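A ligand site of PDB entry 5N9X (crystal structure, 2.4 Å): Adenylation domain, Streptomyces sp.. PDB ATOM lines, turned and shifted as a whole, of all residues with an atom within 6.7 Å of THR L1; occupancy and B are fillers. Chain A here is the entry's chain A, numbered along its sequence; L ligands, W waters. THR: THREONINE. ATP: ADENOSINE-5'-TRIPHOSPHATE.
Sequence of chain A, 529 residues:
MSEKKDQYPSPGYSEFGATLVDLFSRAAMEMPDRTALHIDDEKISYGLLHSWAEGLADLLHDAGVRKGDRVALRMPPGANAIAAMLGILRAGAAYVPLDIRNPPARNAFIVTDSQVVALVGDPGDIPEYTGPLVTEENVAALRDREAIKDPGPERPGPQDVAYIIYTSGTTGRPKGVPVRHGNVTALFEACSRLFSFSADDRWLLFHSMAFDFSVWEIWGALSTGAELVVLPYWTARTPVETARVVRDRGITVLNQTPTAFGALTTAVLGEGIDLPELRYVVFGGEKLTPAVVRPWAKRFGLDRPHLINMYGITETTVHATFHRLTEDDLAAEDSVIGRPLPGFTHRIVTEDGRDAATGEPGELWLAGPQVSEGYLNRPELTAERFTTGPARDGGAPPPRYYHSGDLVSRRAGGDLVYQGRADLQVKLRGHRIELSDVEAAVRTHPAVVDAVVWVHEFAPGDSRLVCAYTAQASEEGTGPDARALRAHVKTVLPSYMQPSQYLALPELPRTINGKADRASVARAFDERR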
ATOM      1  N   PHE A 211      11.485 -19.130  24.029  1.00  0.00           N
ATOM      2  CA  PHE A 211      12.637 -20.024  23.867  1.00  0.00           C
ATOM      3  C   PHE A 211      13.828 -19.192  23.378  1.00  0.00           C
ATOM      4  O   PHE A 211      13.718 -18.435  22.405  1.00  0.00           O
ATOM      5  CB  PHE A 211      12.263 -21.156  22.903  1.00  0.00           C
ATOM      6  CG  PHE A 211      13.365 -22.128  22.644  1.00  0.00           C
ATOM      7  CD1 PHE A 211      14.245 -22.500  23.651  1.00  0.00           C
ATOM      8  CD2 PHE A 211      13.484 -22.732  21.386  1.00  0.00           C
ATOM      9  CE1 PHE A 211      15.261 -23.429  23.410  1.00  0.00           C
ATOM     10  CE2 PHE A 211      14.476 -23.655  21.144  1.00  0.00           C
ATOM     11  CZ  PHE A 211      15.375 -24.005  22.144  1.00  0.00           C
ATOM     12  N   ASP A 212      14.960 -19.309  24.057  1.00  0.00           N
ATOM     13  CA  ASP A 212      16.024 -18.347  23.840  1.00  0.00           C
ATOM     14  C   ASP A 212      16.688 -18.458  22.433  1.00  0.00           C
ATOM     15  O   ASP A 212      17.455 -17.599  22.031  1.00  0.00           O
ATOM     16  CB  ASP A 212      17.037 -18.422  24.995  1.00  0.00           C
ATOM     17  CG  ASP A 212      18.037 -19.556  24.856  1.00  0.00           C
ATOM     18  OD1 ASP A 212      17.828 -20.504  24.067  1.00  0.00           O
ATOM     19  OD2 ASP A 212      19.067 -19.474  25.559  1.00  0.00           O
ATOM     20  N   PHE A 213      16.322 -19.487  21.676  1.00  0.00           N
ATOM     21  CA  PHE A 213      16.812 -19.678  20.316  1.00  0.00           C
ATOM     22  C   PHE A 213      16.217 -18.566  19.402  1.00  0.00           C
ATOM     23  O   PHE A 213      16.791 -18.228  18.365  1.00  0.00           O
ATOM     24  CB  PHE A 213      16.466 -21.134  19.893  1.00  0.00           C
ATOM     25  CG  PHE A 213      17.369 -21.707  18.828  1.00  0.00           C
ATOM     26  CD1 PHE A 213      18.516 -21.039  18.453  1.00  0.00           C
ATOM     27  CD2 PHE A 213      17.195 -23.026  18.379  1.00  0.00           C
ATOM     28  CE1 PHE A 213      19.388 -21.579  17.524  1.00  0.00           C
ATOM     29  CE2 PHE A 213      18.102 -23.611  17.453  1.00  0.00           C
ATOM     30  CZ  PHE A 213      19.193 -22.873  17.026  1.00  0.00           C
ATOM     31  N   TRP A 216      18.591 -15.439  19.296  1.00  0.00           N
ATOM     32  CA  TRP A 216      19.569 -15.594  18.248  1.00  0.00           C
ATOM     33  C   TRP A 216      18.952 -15.231  16.905  1.00  0.00           C
ATOM     34  O   TRP A 216      19.551 -14.528  16.096  1.00  0.00           O
ATOM     35  CB  TRP A 216      20.097 -17.012  18.283  1.00  0.00           C
ATOM     36  CG  TRP A 216      20.889 -17.478  17.144  1.00  0.00           C
ATOM     37  CD1 TRP A 216      20.501 -18.380  16.216  1.00  0.00           C
ATOM     38  CD2 TRP A 216      22.249 -17.118  16.820  1.00  0.00           C
ATOM     39  NE1 TRP A 216      21.515 -18.611  15.324  1.00  0.00           N
ATOM     40  CE2 TRP A 216      22.606 -17.859  15.680  1.00  0.00           C
ATOM     41  CE3 TRP A 216      23.187 -16.247  17.384  1.00  0.00           C
ATOM     42  CZ2 TRP A 216      23.886 -17.742  15.066  1.00  0.00           C
ATOM     43  CZ3 TRP A 216      24.442 -16.133  16.781  1.00  0.00           C
ATOM     44  CH2 TRP A 216      24.777 -16.877  15.642  1.00  0.00           C
ATOM     45  N   THR A 257      16.028 -27.192  15.726  1.00  0.00           N
ATOM     46  CA  THR A 257      16.439 -28.294  16.563  1.00  0.00           C
ATOM     47  C   THR A 257      16.641 -29.490  15.658  1.00  0.00           C
ATOM     48  O   THR A 257      16.130 -29.516  14.547  1.00  0.00           O
ATOM     49  CB  THR A 257      15.442 -28.594  17.652  1.00  0.00           C
ATOM     50  OG1 THR A 257      14.221 -28.973  17.022  1.00  0.00           O
ATOM     51  CG2 THR A 257      15.242 -27.365  18.529  1.00  0.00           C
ATOM     52  N   PHE A 283      22.073 -25.819  14.122  1.00  0.00           N
ATOM     53  CA  PHE A 283      21.336 -26.717  14.996  1.00  0.00           C
ATOM     54  C   PHE A 283      21.582 -26.315  16.433  1.00  0.00           C
ATOM     55  O   PHE A 283      22.717 -25.946  16.788  1.00  0.00           O
ATOM     56  CB  PHE A 283      21.781 -28.174  14.798  1.00  0.00           C
ATOM     57  CG  PHE A 283      21.658 -28.652  13.389  1.00  0.00           C
ATOM     58  CD1 PHE A 283      22.639 -28.354  12.451  1.00  0.00           C
ATOM     59  CD2 PHE A 283      20.558 -29.396  12.993  1.00  0.00           C
ATOM     60  CE1 PHE A 283      22.537 -28.811  11.138  1.00  0.00           C
ATOM     61  CE2 PHE A 283      20.453 -29.868  11.670  1.00  0.00           C
ATOM     62  CZ  PHE A 283      21.441 -29.575  10.747  1.00  0.00           C
ATOM     63  N   GLY A 284      20.561 -26.431  17.259  1.00  0.00           N
ATOM     64  CA  GLY A 284      20.769 -26.271  18.684  1.00  0.00           C
ATOM     65  C   GLY A 284      19.760 -26.986  19.549  1.00  0.00           C
ATOM     66  O   GLY A 284      18.643 -27.269  19.117  1.00  0.00           O
ATOM     67  N   GLY A 285      20.144 -27.274  20.778  1.00  0.00           N
ATOM     68  CA  GLY A 285      19.182 -27.631  21.794  1.00  0.00           C
ATOM     69  C   GLY A 285      19.052 -29.115  22.063  1.00  0.00           C
ATOM     70  O   GLY A 285      18.478 -29.492  23.074  1.00  0.00           O
ATOM     71  N   GLU A 286      19.554 -29.954  21.157  1.00  0.00           N
ATOM     72  CA  GLU A 286      19.471 -31.409  21.318  1.00  0.00           C
ATOM     73  C   GLU A 286      20.738 -32.022  20.815  1.00  0.00           C
ATOM     74  O   GLU A 286      21.499 -31.359  20.102  1.00  0.00           O
ATOM     75  CB  GLU A 286      18.290 -32.000  20.549  1.00  0.00           C
ATOM     76  CG  GLU A 286      16.992 -31.286  20.758  1.00  0.00           C
ATOM     77  CD  GLU A 286      15.806 -32.060  20.238  1.00  0.00           C
ATOM     78  OE1 GLU A 286      15.793 -32.448  19.042  1.00  0.00           O
ATOM     79  OE2 GLU A 286      14.863 -32.254  21.038  1.00  0.00           O
ATOM     80  N   MET A 310      25.499 -26.301  17.236  1.00  0.00           N
ATOM     81  CA  MET A 310      25.899 -25.447  18.359  1.00  0.00           C
ATOM     82  C   MET A 310      25.365 -26.004  19.674  1.00  0.00           C
ATOM     83  O   MET A 310      24.152 -26.119  19.847  1.00  0.00           O
ATOM     84  CB  MET A 310      25.428 -24.001  18.165  1.00  0.00           C
ATOM     85  CG  MET A 310      26.050 -23.315  16.955  1.00  0.00           C
ATOM     86  SD  MET A 310      25.700 -21.536  16.748  1.00  0.00           S
ATOM     87  CE  MET A 310      27.074 -20.819  17.695  1.00  0.00           C
ATOM     88  N   TYR A 311      26.273 -26.369  20.580  1.00  0.00           N
ATOM     89  CA  TYR A 311      25.854 -26.717  21.928  1.00  0.00           C
ATOM     90  C   TYR A 311      25.559 -25.416  22.633  1.00  0.00           C
ATOM     91  O   TYR A 311      26.305 -24.436  22.443  1.00  0.00           O
ATOM     92  CB  TYR A 311      26.928 -27.528  22.690  1.00  0.00           C
ATOM     93  CG  TYR A 311      26.673 -27.623  24.198  1.00  0.00           C
ATOM     94  CD1 TYR A 311      25.882 -28.634  24.710  1.00  0.00           C
ATOM     95  CD2 TYR A 311      27.245 -26.721  25.089  1.00  0.00           C
ATOM     96  CE1 TYR A 311      25.659 -28.736  26.065  1.00  0.00           C
ATOM     97  CE2 TYR A 311      27.019 -26.814  26.441  1.00  0.00           C
ATOM     98  CZ  TYR A 311      26.216 -27.815  26.922  1.00  0.00           C
ATOM     99  OH  TYR A 311      25.993 -27.900  28.263  1.00  0.00           O
ATOM    100  N   GLY A 312      24.495 -25.412  23.425  1.00  0.00           N
ATOM    101  CA  GLY A 312      24.111 -24.207  24.142  1.00  0.00           C
ATOM    102  C   GLY A 312      23.193 -24.518  25.292  1.00  0.00           C
ATOM    103  O   GLY A 312      22.554 -25.585  25.337  1.00  0.00           O
ATOM    104  N   ILE A 313      23.139 -23.590  26.244  1.00  0.00           N
ATOM    105  CA  ILE A 313      22.233 -23.627  27.389  1.00  0.00           C
ATOM    106  C   ILE A 313      21.765 -22.228  27.655  1.00  0.00           C
ATOM    107  O   ILE A 313      22.485 -21.274  27.357  1.00  0.00           O
ATOM    108  CB  ILE A 313      22.920 -24.159  28.653  1.00  0.00           C
ATOM    109  CG1 ILE A 313      24.407 -23.862  28.582  1.00  0.00           C
ATOM    110  CG2 ILE A 313      22.661 -25.627  28.869  1.00  0.00           C
ATOM    111  CD1 ILE A 313      25.200 -24.454  29.684  1.00  0.00           C
ATOM    112  N   THR A 314      20.570 -22.087  28.233  1.00  0.00           N
ATOM    113  CA  THR A 314      19.998 -20.771  28.457  1.00  0.00           C
ATOM    114  C   THR A 314      20.846 -19.970  29.454  1.00  0.00           C
ATOM    115  O   THR A 314      20.953 -18.735  29.360  1.00  0.00           O
ATOM    116  CB  THR A 314      18.521 -20.867  28.963  1.00  0.00           C
ATOM    117  OG1 THR A 314      17.703 -21.486  27.954  1.00  0.00           O
ATOM    118  CG2 THR A 314      17.971 -19.491  29.308  1.00  0.00           C
ATOM    119  N   GLU A 315      21.508 -20.683  30.361  1.00  0.00           N
ATOM    120  CA  GLU A 315      22.326 -20.058  31.391  1.00  0.00           C
ATOM    121  C   GLU A 315      23.593 -19.393  30.860  1.00  0.00           C
ATOM    122  O   GLU A 315      24.223 -18.611  31.556  1.00  0.00           O
ATOM    123  CB  GLU A 315      22.676 -21.085  32.488  1.00  0.00           C
ATOM    124  CG  GLU A 315      21.489 -21.520  33.369  1.00  0.00           C
ATOM    125  CD  GLU A 315      20.645 -22.662  32.794  1.00  0.00           C
ATOM    126  OE1 GLU A 315      20.766 -23.007  31.595  1.00  0.00           O
ATOM    127  OE2 GLU A 315      19.839 -23.211  33.563  1.00  0.00           O
ATOM    128  N   THR A 317      23.587 -18.006  27.580  1.00  0.00           N
ATOM    129  CA  THR A 317      23.056 -17.185  26.497  1.00  0.00           C
ATOM    130  C   THR A 317      23.039 -17.879  25.116  1.00  0.00           C
ATOM    131  O   THR A 317      23.853 -17.576  24.255  1.00  0.00           O
ATOM    132  CB  THR A 317      23.804 -15.823  26.387  1.00  0.00           C
ATOM    133  OG1 THR A 317      24.093 -15.313  27.698  1.00  0.00           O
ATOM    134  CG2 THR A 317      22.981 -14.789  25.595  1.00  0.00           C
ATOM    135  N   VAL A 318      22.050 -18.747  24.921  1.00  0.00           N
ATOM    136  CA  VAL A 318      21.753 -19.396  23.646  1.00  0.00           C
ATOM    137  C   VAL A 318      22.777 -20.425  23.126  1.00  0.00           C
ATOM    138  O   VAL A 318      22.418 -21.598  22.998  1.00  0.00           O
ATOM    139  CB  VAL A 318      21.503 -18.361  22.516  1.00  0.00           C
ATOM    140  CG1 VAL A 318      20.714 -19.005  21.402  1.00  0.00           C
ATOM    141  CG2 VAL A 318      20.739 -17.126  23.048  1.00  0.00           C
ATOM    142  N   HIS A 319      24.003 -20.009  22.817  1.00  0.00           N
ATOM    143  CA  HIS A 319      25.053 -20.905  22.304  1.00  0.00           C
ATOM    144  C   HIS A 319      26.347 -20.848  23.092  1.00  0.00           C
ATOM    145  O   HIS A 319      26.746 -19.783  23.553  1.00  0.00           O
ATOM    146  CB  HIS A 319      25.375 -20.612  20.821  1.00  0.00           C
ATOM    147  CG  HIS A 319      24.164 -20.447  19.949  1.00  0.00           C
ATOM    148  ND1 HIS A 319      23.276 -21.465  19.720  1.00  0.00           N
ATOM    149  CD2 HIS A 319      23.708 -19.378  19.244  1.00  0.00           C
ATOM    150  CE1 HIS A 319      22.320 -21.038  18.913  1.00  0.00           C
ATOM    151  NE2 HIS A 319      22.563 -19.777  18.608  1.00  0.00           N
ATOM    152  N   ALA A 320      27.040 -21.980  23.179  1.00  0.00           N
ATOM    153  CA  ALA A 320      28.294 -22.043  23.905  1.00  0.00           C
ATOM    154  C   ALA A 320      29.430 -22.668  23.073  1.00  0.00           C
ATOM    155  O   ALA A 320      30.608 -22.594  23.476  1.00  0.00           O
ATOM    156  CB  ALA A 320      28.109 -22.835  25.185  1.00  0.00           C
ATOM    157  N   ASN A 513       9.652 -25.071  23.376  1.00  0.00           N
ATOM    158  CA  ASN A 513      10.888 -25.097  22.590  1.00  0.00           C
ATOM    159  C   ASN A 513      10.974 -26.276  21.627  1.00  0.00           C
ATOM    160  O   ASN A 513      12.034 -26.543  21.056  1.00  0.00           O
ATOM    161  CB  ASN A 513      12.105 -25.129  23.517  1.00  0.00           C
ATOM    162  CG  ASN A 513      12.187 -26.406  24.381  1.00  0.00           C
ATOM    163  OD1 ASN A 513      11.353 -27.308  24.267  1.00  0.00           O
ATOM    164  ND2 ASN A 513      13.196 -26.472  25.240  1.00  0.00           N
ATOM    165  N   LYS A 515      11.180 -29.445  22.290  1.00  0.00           N
ATOM    166  CA  LYS A 515      11.737 -30.688  22.842  1.00  0.00           C
ATOM    167  C   LYS A 515      10.667 -31.597  23.472  1.00  0.00           C
ATOM    168  O   LYS A 515       9.568 -31.141  23.840  1.00  0.00           O
ATOM    169  CB  LYS A 515      12.823 -30.393  23.887  1.00  0.00           C
ATOM    170  CG  LYS A 515      14.015 -29.648  23.348  1.00  0.00           C
ATOM    171  CD  LYS A 515      14.926 -29.185  24.456  1.00  0.00           C
ATOM    172  CE  LYS A 515      15.852 -28.086  23.989  1.00  0.00           C
ATOM    173  NZ  LYS A 515      16.844 -27.716  25.019  1.00  0.00           N
HETATM  174  N   THR L   1      19.702 -22.376  24.143  1.00  0.00           N
HETATM  175  CA  THR L   1      18.874 -23.379  23.456  1.00  0.00           C
HETATM  176  C   THR L   1      18.595 -24.457  24.458  1.00  0.00           C
HETATM  177  O   THR L   1      17.785 -25.405  24.319  1.00  0.00           O
HETATM  178  CB  THR L   1      19.580 -24.011  22.232  1.00  0.00           C
HETATM  179  OG1 THR L   1      20.920 -24.429  22.588  1.00  0.00           O
HETATM  180  CG2 THR L   1      19.634 -23.016  21.074  1.00  0.00           C
HETATM  181  OXT THR L   1      19.274 -24.335  25.471  1.00  0.00           O
HETATM  182  PG  ATP L   2      17.292 -26.463  32.051  1.00  0.00           P
HETATM  183  O1G ATP L   2      18.477 -27.331  32.472  1.00  0.00           O
HETATM  184  O2G ATP L   2      16.172 -26.441  33.049  1.00  0.00           O
HETATM  185  O3G ATP L   2      17.663 -25.049  31.651  1.00  0.00           O
HETATM  186  PB  ATP L   2      17.097 -27.220  29.239  1.00  0.00           P
HETATM  187  O1B ATP L   2      18.312 -28.153  29.305  1.00  0.00           O
HETATM  188  O2B ATP L   2      16.056 -27.426  28.185  1.00  0.00           O
HETATM  189  O3B ATP L   2      16.565 -27.207  30.773  1.00  0.00           O
HETATM  190  PA  ATP L   2      18.025 -25.005  27.845  1.00  0.00           P
HETATM  191  O1A ATP L   2      19.086 -24.005  28.237  1.00  0.00           O
HETATM  192  O2A ATP L   2      16.879 -24.530  26.950  1.00  0.00           O
HETATM  193  O3A ATP L   2      17.471 -25.661  29.193  1.00  0.00           O
HETATM  194  O5' ATP L   2      18.644 -26.376  27.217  1.00  0.00           O
HETATM  195  C5' ATP L   2      20.028 -26.677  27.108  1.00  0.00           C
HETATM  196  C4' ATP L   2      20.251 -28.193  27.167  1.00  0.00           C
HETATM  197  O4' ATP L   2      20.060 -28.791  25.897  1.00  0.00           O
HETATM  198  C3' ATP L   2      21.622 -28.625  27.675  1.00  0.00           C
HETATM  199  O3' ATP L   2      21.432 -29.087  29.008  1.00  0.00           O
HETATM  200  C2' ATP L   2      22.055 -29.756  26.786  1.00  0.00           C
HETATM  201  O2' ATP L   2      21.853 -30.981  27.485  1.00  0.00           O
HETATM  202  C1' ATP L   2      21.101 -29.731  25.603  1.00  0.00           C
HETATM  203  N9  ATP L   2      21.796 -29.309  24.347  1.00  0.00           N
HETATM  204  C8  ATP L   2      21.766 -28.064  23.817  1.00  0.00           C
HETATM  205  N7  ATP L   2      22.477 -27.967  22.669  1.00  0.00           N
HETATM  206  C5  ATP L   2      22.975 -29.195  22.427  1.00  0.00           C
HETATM  207  C6  ATP L   2      23.819 -29.790  21.361  1.00  0.00           C
HETATM  208  N6  ATP L   2      24.253 -29.028  20.340  1.00  0.00           N
HETATM  209  N1  ATP L   2      24.130 -31.089  21.462  1.00  0.00           N
HETATM  210  C2  ATP L   2      23.711 -31.820  22.506  1.00  0.00           C
HETATM  211  N3  ATP L   2      22.922 -31.369  23.515  1.00  0.00           N
HETATM  212  C4  ATP L   2      22.528 -30.071  23.534  1.00  0.00           C
HETATM  213  O   HOH W   1      22.925 -24.134  21.063  1.00  0.00           O
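An oxygen (O5') of ATP L2 lies close to an oxygen (OXT) of THR L1, 2.8 Å away.
NZ of Lys 515 sits at hydrogen-bond distance from O of Gly 285, 3.1 Å away. The backbone NH of Val 318 sits at hydrogen-bond distance from the side-chain carboxylate of Asp 212, at 3.1 Å. The side-chain amide oxygen of Asn 513 is in hydrogen-bond range of the backbone NH of Lys 515 (2.9 Å). The side-chain carboxylate (OD2) of Asp 212 sits close to the side-chain hydroxyl (OG1) of Thr 314 (3.4 Å).
CE1 of Phe 211 touches O of THR L1, 3.3 Å away. Phe 213 touches THR L1 (CG to CG2, 3.4 Å). Ile 313 touches THR L1 (CA to OXT, 3.6 Å). Thr 314 touches THR L1 (N to OXT, 3.8 Å). His 319 touches THR L1 (CE1 to CG2, 3.97 Å). Hydrophobic or aromatic side chains that line THR L1: Phe 211, Phe 213 and His 319.
An oxygen (O) of THR L1 is in salt-bridge range of the side-chain amino group (NZ) of Lys 515, at 2.6 Å. The backbone NH (N) of Gly 285 sits at hydrogen-bond distance from a nitrogen (N7) of ATP L2 (3.1 Å). O of Val 318 sits at hydrogen-bond distance from N of THR L1, 3.0 Å away. OD1 of Asp 212 lies within salt-bridge range of N of THR L1 (2.6 Å). N of Thr 314 lies within hydrogen-bond range of O1A of ATP L2, at 2.4 Å. The backbone NH of Gly 312 lies within hydrogen-bond range of a nitrogen (N7) of ATP L2 (3.3 Å). The backbone NH of Gly 285 sits at hydrogen-bond distance from an oxygen (OG1) of THR L1 (3.5 Å). The side-chain hydroxyl (OG1) of Thr 314 sits at hydrogen-bond distance from an oxygen (O1A) of ATP L2 (2.9 Å). The backbone carbonyl oxygen (O) of Met 310 is in hydrogen-bond range of a nitrogen (N6) of ATP L2, 3.0 Å away. O of Gly 312 is in hydrogen-bond range of OG1 of THR L1 (3.4 Å). The side-chain amino group of Lys 515 lies within salt-bridge range of an oxygen (O2B) of ATP L2, 3.3 Å away.
Water W1 lies within hydrogen-bond range of OG1 of THR L1 (2.5 Å), O of Met 310 (2.6 Å), ND1 of His 319 (3.0 Å), N of Gly 312 (3.1 Å) and O of Val 318 (3.2 Å).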
